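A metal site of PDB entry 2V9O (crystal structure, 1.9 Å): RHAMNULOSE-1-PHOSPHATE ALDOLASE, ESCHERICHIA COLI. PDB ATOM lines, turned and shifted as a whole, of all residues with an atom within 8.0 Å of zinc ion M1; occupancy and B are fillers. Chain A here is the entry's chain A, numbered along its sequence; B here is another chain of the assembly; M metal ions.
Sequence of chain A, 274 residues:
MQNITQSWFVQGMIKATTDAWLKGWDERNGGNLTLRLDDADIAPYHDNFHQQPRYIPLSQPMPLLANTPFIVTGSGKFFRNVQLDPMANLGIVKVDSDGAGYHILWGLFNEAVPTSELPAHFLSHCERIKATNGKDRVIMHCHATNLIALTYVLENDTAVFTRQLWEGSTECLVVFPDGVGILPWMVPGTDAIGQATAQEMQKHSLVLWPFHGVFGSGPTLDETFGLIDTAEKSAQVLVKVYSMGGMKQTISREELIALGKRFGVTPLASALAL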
ATOM      1  N   TRP A  25      27.771 -30.652  28.422  1.00  0.00           N
ATOM      2  CA  TRP A  25      26.708 -30.046  27.642  1.00  0.00           C
ATOM      3  C   TRP A  25      25.314 -30.234  28.166  1.00  0.00           C
ATOM      4  O   TRP A  25      24.382 -29.687  27.613  1.00  0.00           O
ATOM      5  CB  TRP A  25      26.704 -30.523  26.194  1.00  0.00           C
ATOM      6  CG  TRP A  25      28.071 -30.264  25.428  1.00  0.00           C
ATOM      7  CD1 TRP A  25      29.138 -29.512  25.823  1.00  0.00           C
ATOM      8  CD2 TRP A  25      28.398 -30.802  24.126  1.00  0.00           C
ATOM      9  NE1 TRP A  25      30.169 -29.603  24.862  1.00  0.00           N
ATOM     10  CE2 TRP A  25      29.719 -30.393  23.825  1.00  0.00           C
ATOM     11  CE3 TRP A  25      27.743 -31.697  23.266  1.00  0.00           C
ATOM     12  CZ2 TRP A  25      30.372 -30.787  22.639  1.00  0.00           C
ATOM     13  CZ3 TRP A  25      28.375 -32.080  22.041  1.00  0.00           C
ATOM     14  CH2 TRP A  25      29.663 -31.643  21.770  1.00  0.00           C
ATOM     15  N   ASP A  26      25.143 -31.033  29.211  1.00  0.00           N
ATOM     16  CA  ASP A  26      23.792 -31.480  29.465  1.00  0.00           C
ATOM     17  C   ASP A  26      23.572 -31.640  30.970  1.00  0.00           C
ATOM     18  O   ASP A  26      23.288 -32.718  31.474  1.00  0.00           O
ATOM     19  CB  ASP A  26      23.593 -32.745  28.692  1.00  0.00           C
ATOM     20  CG  ASP A  26      23.382 -32.488  27.175  1.00  0.00           C
ATOM     21  OD1 ASP A  26      24.315 -32.722  26.407  1.00  0.00           O
ATOM     22  OD2 ASP A  26      22.268 -32.031  26.776  1.00  0.00           O
ATOM     23  N   GLU A  27      23.810 -30.538  31.680  1.00  0.00           N
ATOM     24  CA  GLU A  27      23.548 -30.350  33.117  1.00  0.00           C
ATOM     25  C   GLU A  27      22.054 -30.674  33.312  1.00  0.00           C
ATOM     26  O   GLU A  27      21.263 -30.449  32.398  1.00  0.00           O
ATOM     27  CB  GLU A  27      23.816 -28.896  33.526  1.00  0.00           C
ATOM     28  CG  GLU A  27      22.733 -27.799  33.051  1.00  0.00           C
ATOM     29  CD  GLU A  27      22.891 -27.317  31.613  1.00  0.00           C
ATOM     30  OE1 GLU A  27      22.074 -26.430  31.126  1.00  0.00           O
ATOM     31  OE2 GLU A  27      23.867 -27.794  30.986  1.00  0.00           O
ATOM     32  N   ASN A  29      18.360 -31.865  33.257  1.00  0.00           N
ATOM     33  CA  ASN A  29      17.701 -32.357  32.004  1.00  0.00           C
ATOM     34  C   ASN A  29      18.014 -31.566  30.752  1.00  0.00           C
ATOM     35  O   ASN A  29      17.200 -31.625  29.794  1.00  0.00           O
ATOM     36  CB  ASN A  29      16.146 -32.318  32.123  1.00  0.00           C
ATOM     37  CG  ASN A  29      15.619 -30.973  32.458  1.00  0.00           C
ATOM     38  OD1 ASN A  29      15.866 -30.479  33.552  1.00  0.00           O
ATOM     39  ND2 ASN A  29      14.846 -30.365  31.542  1.00  0.00           N
ATOM     40  N   GLY A  30      19.066 -30.753  30.783  1.00  0.00           N
ATOM     41  CA  GLY A  30      19.321 -29.818  29.707  1.00  0.00           C
ATOM     42  C   GLY A  30      19.615 -30.542  28.417  1.00  0.00           C
ATOM     43  O   GLY A  30      20.415 -31.459  28.385  1.00  0.00           O
ATOM     44  N   GLY A  31      19.045 -30.115  27.300  1.00  0.00           N
ATOM     45  CA  GLY A  31      19.484 -30.711  26.026  1.00  0.00           C
ATOM     46  C   GLY A  31      18.422 -31.735  25.696  1.00  0.00           C
ATOM     47  O   GLY A  31      17.728 -32.237  26.581  1.00  0.00           O
ATOM     48  N   ASN A  32      18.274 -32.094  24.429  1.00  0.00           N
ATOM     49  CA  ASN A  32      17.391 -33.191  24.083  1.00  0.00           C
ATOM     50  C   ASN A  32      17.737 -33.716  22.710  1.00  0.00           C
ATOM     51  O   ASN A  32      18.456 -33.063  22.015  1.00  0.00           O
ATOM     52  CB  ASN A  32      15.918 -32.683  24.132  1.00  0.00           C
ATOM     53  CG  ASN A  32      15.828 -31.118  24.011  1.00  0.00           C
ATOM     54  OD1 ASN A  32      15.881 -30.566  22.906  1.00  0.00           O
ATOM     55  ND2 ASN A  32      15.748 -30.428  25.192  1.00  0.00           N
ATOM     56  N   THR A 115      10.504 -35.115  25.226  1.00  0.00           N
ATOM     57  CA  THR A 115      11.022 -33.757  25.456  1.00  0.00           C
ATOM     58  C   THR A 115      10.079 -32.565  25.260  1.00  0.00           C
ATOM     59  O   THR A 115       9.243 -32.519  24.298  1.00  0.00           O
ATOM     60  CB  THR A 115      12.276 -33.500  24.665  1.00  0.00           C
ATOM     61  OG1 THR A 115      12.821 -32.258  25.071  1.00  0.00           O
ATOM     62  CG2 THR A 115      12.003 -33.536  23.167  1.00  0.00           C
ATOM     63  N   SER A 116      10.199 -31.602  26.184  1.00  0.00           N
ATOM     64  CA  SER A 116       9.390 -30.374  26.119  1.00  0.00           C
ATOM     65  C   SER A 116       9.824 -29.488  24.925  1.00  0.00           C
ATOM     66  O   SER A 116       9.106 -28.539  24.580  1.00  0.00           O
ATOM     67  CB  SER A 116       9.459 -29.620  27.448  1.00  0.00           C
ATOM     68  OG  SER A 116      10.794 -29.185  27.597  1.00  0.00           O
ATOM     69  N   GLU A 117      10.935 -29.829  24.265  1.00  0.00           N
ATOM     70  CA  GLU A 117      11.302 -29.138  23.025  1.00  0.00           C
ATOM     71  C   GLU A 117      10.822 -29.884  21.797  1.00  0.00           C
ATOM     72  O   GLU A 117      11.297 -29.589  20.713  1.00  0.00           O
ATOM     73  CB  GLU A 117      12.799 -28.864  22.862  1.00  0.00           C
ATOM     74  CG  GLU A 117      13.438 -28.061  23.989  1.00  0.00           C
ATOM     75  CD  GLU A 117      13.026 -26.623  24.013  1.00  0.00           C
ATOM     76  OE1 GLU A 117      13.599 -25.957  24.880  1.00  0.00           O
ATOM     77  OE2 GLU A 117      12.161 -26.155  23.200  1.00  0.00           O
ATOM     78  N   HIS A 141      19.902 -31.114  20.511  1.00  0.00           N
ATOM     79  CA  HIS A 141      20.015 -29.859  21.209  1.00  0.00           C
ATOM     80  C   HIS A 141      20.813 -30.124  22.466  1.00  0.00           C
ATOM     81  O   HIS A 141      20.499 -31.096  23.267  1.00  0.00           O
ATOM     82  CB  HIS A 141      18.608 -29.282  21.572  1.00  0.00           C
ATOM     83  CG  HIS A 141      18.613 -28.198  22.626  1.00  0.00           C
ATOM     84  ND1 HIS A 141      19.326 -27.031  22.486  1.00  0.00           N
ATOM     85  CD2 HIS A 141      17.918 -28.042  23.797  1.00  0.00           C
ATOM     86  CE1 HIS A 141      19.087 -26.222  23.507  1.00  0.00           C
ATOM     87  NE2 HIS A 141      18.223 -26.801  24.315  1.00  0.00           N
ATOM     88  N   CYS A 142      21.854 -29.299  22.658  1.00  0.00           N
ATOM     89  CA  CYS A 142      22.613 -29.384  23.917  1.00  0.00           C
ATOM     90  C   CYS A 142      23.077 -28.043  24.372  1.00  0.00           C
ATOM     91  O   CYS A 142      23.127 -27.134  23.608  1.00  0.00           O
ATOM     92  CB  CYS A 142      23.860 -30.268  23.730  1.00  0.00           C
ATOM     93  SG  CYS A 142      24.907 -29.733  22.404  1.00  0.00           S
ATOM     94  N   HIS A 143      23.417 -27.921  25.652  1.00  0.00           N
ATOM     95  CA  HIS A 143      23.848 -26.653  26.142  1.00  0.00           C
ATOM     96  C   HIS A 143      25.397 -26.549  26.016  1.00  0.00           C
ATOM     97  O   HIS A 143      26.100 -26.721  27.022  1.00  0.00           O
ATOM     98  CB  HIS A 143      23.387 -26.553  27.564  1.00  0.00           C
ATOM     99  CG  HIS A 143      21.892 -26.525  27.670  1.00  0.00           C
ATOM    100  ND1 HIS A 143      21.214 -26.503  28.868  1.00  0.00           N
ATOM    101  CD2 HIS A 143      20.955 -26.533  26.706  1.00  0.00           C
ATOM    102  CE1 HIS A 143      19.897 -26.417  28.620  1.00  0.00           C
ATOM    103  NE2 HIS A 143      19.737 -26.492  27.319  1.00  0.00           N
ATOM    104  N   ILE A 148      27.560 -21.185  24.049  1.00  0.00           N
ATOM    105  CA  ILE A 148      26.598 -20.368  24.787  1.00  0.00           C
ATOM    106  C   ILE A 148      27.378 -19.074  25.218  1.00  0.00           C
ATOM    107  O   ILE A 148      26.855 -17.956  25.184  1.00  0.00           O
ATOM    108  CB  ILE A 148      26.203 -21.165  26.034  1.00  0.00           C
ATOM    109  CG1 ILE A 148      25.271 -22.305  25.672  1.00  0.00           C
ATOM    110  CG2 ILE A 148      25.540 -20.245  27.141  1.00  0.00           C
ATOM    111  CD1 ILE A 148      25.007 -23.314  26.844  1.00  0.00           C
ATOM    112  N   PRO A 188      11.778 -20.755  25.604  1.00  0.00           N
ATOM    113  CA  PRO A 188      11.926 -22.076  25.087  1.00  0.00           C
ATOM    114  C   PRO A 188      10.679 -22.975  25.410  1.00  0.00           C
ATOM    115  O   PRO A 188       9.847 -22.608  26.296  1.00  0.00           O
ATOM    116  CB  PRO A 188      13.196 -22.522  25.767  1.00  0.00           C
ATOM    117  CG  PRO A 188      13.174 -21.823  27.104  1.00  0.00           C
ATOM    118  CD  PRO A 188      12.602 -20.528  26.833  1.00  0.00           C
ATOM    119  N   GLY A 189      10.515 -24.044  24.615  1.00  0.00           N
ATOM    120  CA  GLY A 189       9.620 -25.130  24.890  1.00  0.00           C
ATOM    121  C   GLY A 189       8.248 -24.726  24.388  1.00  0.00           C
ATOM    122  O   GLY A 189       7.250 -25.249  24.899  1.00  0.00           O
ATOM    123  N   TRP A 209      20.545 -20.723  19.934  1.00  0.00           N
ATOM    124  CA  TRP A 209      19.636 -20.100  20.810  1.00  0.00           C
ATOM    125  C   TRP A 209      20.531 -19.354  21.746  1.00  0.00           C
ATOM    126  O   TRP A 209      21.058 -19.979  22.665  1.00  0.00           O
ATOM    127  CB  TRP A 209      18.890 -21.202  21.570  1.00  0.00           C
ATOM    128  CG  TRP A 209      17.833 -21.912  20.731  1.00  0.00           C
ATOM    129  CD1 TRP A 209      17.663 -21.858  19.353  1.00  0.00           C
ATOM    130  CD2 TRP A 209      16.856 -22.818  21.212  1.00  0.00           C
ATOM    131  NE1 TRP A 209      16.655 -22.628  18.996  1.00  0.00           N
ATOM    132  CE2 TRP A 209      16.100 -23.202  20.108  1.00  0.00           C
ATOM    133  CE3 TRP A 209      16.508 -23.297  22.479  1.00  0.00           C
ATOM    134  CZ2 TRP A 209      15.007 -24.050  20.211  1.00  0.00           C
ATOM    135  CZ3 TRP A 209      15.394 -24.142  22.572  1.00  0.00           C
ATOM    136  CH2 TRP A 209      14.682 -24.504  21.456  1.00  0.00           C
ATOM    137  N   PHE A 211      22.247 -17.577  24.720  1.00  0.00           N
ATOM    138  CA  PHE A 211      22.124 -17.636  26.174  1.00  0.00           C
ATOM    139  C   PHE A 211      21.398 -18.938  26.562  1.00  0.00           C
ATOM    140  O   PHE A 211      20.908 -19.096  27.669  1.00  0.00           O
ATOM    141  CB  PHE A 211      21.438 -16.396  26.814  1.00  0.00           C
ATOM    142  CG  PHE A 211      21.611 -15.082  26.031  1.00  0.00           C
ATOM    143  CD1 PHE A 211      20.494 -14.316  25.687  1.00  0.00           C
ATOM    144  CD2 PHE A 211      22.881 -14.607  25.669  1.00  0.00           C
ATOM    145  CE1 PHE A 211      20.623 -13.135  24.934  1.00  0.00           C
ATOM    146  CE2 PHE A 211      23.037 -13.399  24.934  1.00  0.00           C
ATOM    147  CZ  PHE A 211      21.887 -12.691  24.554  1.00  0.00           C
ATOM    148  N   HIS A 212      21.452 -19.891  25.639  1.00  0.00           N
ATOM    149  CA  HIS A 212      20.810 -21.154  25.921  1.00  0.00           C
ATOM    150  C   HIS A 212      21.497 -22.410  25.362  1.00  0.00           C
ATOM    151  O   HIS A 212      22.017 -23.258  26.113  1.00  0.00           O
ATOM    152  CB  HIS A 212      19.433 -21.032  25.284  1.00  0.00           C
ATOM    153  CG  HIS A 212      18.543 -22.156  25.611  1.00  0.00           C
ATOM    154  ND1 HIS A 212      17.154 -22.038  25.687  1.00  0.00           N
ATOM    155  CD2 HIS A 212      18.832 -23.461  25.727  1.00  0.00           C
ATOM    156  CE1 HIS A 212      16.656 -23.234  25.968  1.00  0.00           C
ATOM    157  NE2 HIS A 212      17.672 -24.102  26.032  1.00  0.00           N
ATOM    158  N   GLY A 213      21.442 -22.576  24.030  1.00  0.00           N
ATOM    159  CA  GLY A 213      22.226 -23.677  23.457  1.00  0.00           C
ATOM    160  C   GLY A 213      22.322 -23.698  21.949  1.00  0.00           C
ATOM    161  O   GLY A 213      22.200 -22.647  21.327  1.00  0.00           O
ATOM    162  N   VAL A 214      22.574 -24.878  21.379  1.00  0.00           N
ATOM    163  CA  VAL A 214      22.643 -25.063  19.941  1.00  0.00           C
ATOM    164  C   VAL A 214      21.742 -26.259  19.581  1.00  0.00           C
ATOM    165  O   VAL A 214      21.458 -27.132  20.425  1.00  0.00           O
ATOM    166  CB  VAL A 214      24.068 -25.240  19.506  1.00  0.00           C
ATOM    167  CG1 VAL A 214      24.615 -26.565  20.041  1.00  0.00           C
ATOM    168  CG2 VAL A 214      24.290 -25.181  18.017  1.00  0.00           C
ATOM    169  N   PHE A 215      21.239 -26.227  18.362  1.00  0.00           N
ATOM    170  CA  PHE A 215      20.432 -27.233  17.726  1.00  0.00           C
ATOM    171  C   PHE A 215      21.262 -27.590  16.499  1.00  0.00           C
ATOM    172  O   PHE A 215      21.814 -26.690  15.870  1.00  0.00           O
ATOM    173  CB  PHE A 215      19.070 -26.674  17.285  1.00  0.00           C
ATOM    174  CG  PHE A 215      17.976 -26.981  18.221  1.00  0.00           C
ATOM    175  CD1 PHE A 215      17.828 -26.261  19.373  1.00  0.00           C
ATOM    176  CD2 PHE A 215      17.144 -28.057  18.021  1.00  0.00           C
ATOM    177  CE1 PHE A 215      16.781 -26.587  20.287  1.00  0.00           C
ATOM    178  CE2 PHE A 215      16.188 -28.388  18.951  1.00  0.00           C
ATOM    179  CZ  PHE A 215      15.985 -27.682  20.066  1.00  0.00           C
ATOM    180  N   THR B 170      19.743 -19.994  30.165  1.00  0.00           N
ATOM    181  CA  THR B 170      18.319 -19.712  30.153  1.00  0.00           C
ATOM    182  C   THR B 170      17.423 -20.405  31.170  1.00  0.00           C
ATOM    183  O   THR B 170      16.488 -19.797  31.727  1.00  0.00           O
ATOM    184  CB  THR B 170      17.696 -19.913  28.782  1.00  0.00           C
ATOM    185  OG1 THR B 170      18.172 -18.872  27.909  1.00  0.00           O
ATOM    186  CG2 THR B 170      16.172 -19.759  28.873  1.00  0.00           C
ATOM    187  N   GLU B 171      17.665 -21.707  31.368  1.00  0.00           N
ATOM    188  CA  GLU B 171      16.906 -22.619  32.199  1.00  0.00           C
ATOM    189  C   GLU B 171      16.966 -22.351  33.696  1.00  0.00           C
ATOM    190  O   GLU B 171      16.307 -22.970  34.455  1.00  0.00           O
ATOM    191  CB  GLU B 171      17.567 -23.973  31.947  1.00  0.00           C
ATOM    192  CG  GLU B 171      19.064 -23.895  31.415  1.00  0.00           C
ATOM    193  CD  GLU B 171      19.998 -24.816  32.168  1.00  0.00           C
ATOM    194  OE1 GLU B 171      19.798 -26.042  32.175  1.00  0.00           O
ATOM    195  OE2 GLU B 171      20.946 -24.324  32.784  1.00  0.00           O
HETATM  196 ZN    ZN M   1      17.789 -26.276  26.255  1.00  0.00          ZN
HETATM  197 ZN    ZN M   2      13.722 -31.570  28.337  1.00  0.00          ZN
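The backbone NH (N) of Asn 32 is in hydrogen-bond range of the backbone carbonyl oxygen (O) of His 141, at 2.7 Å.
The backbone carbonyl oxygen (O) of Val 214 lies within hydrogen-bond range of a ring nitrogen (ND1) of His 141, 3.0 Å away.
The side-chain carboxylate of Glu 27 sits at hydrogen-bond distance from a ring nitrogen (ND1) of His 143, 2.4 Å away.
The backbone NH (N) of His 143 lies within hydrogen-bond range of the backbone carbonyl oxygen (O) of Trp 25 (2.8 Å).
Three residues have an atom within 4 Å of zinc ion M1: His 141, His 143 and His 212.
Along chain A the residues within 4 Å of zinc ion M1 span positions 141 to 212.
The nearest printed residue that does not touch zinc ion M1 is Gly 31 (4.2 Å).
Zinc ion M1 is bound by a ring nitrogen (NE2) of His 141 (2.1 Å), a ring nitrogen (NE2) of His 212 (2.2 Å) and a ring nitrogen (NE2) of His 143 (2.2 Å).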
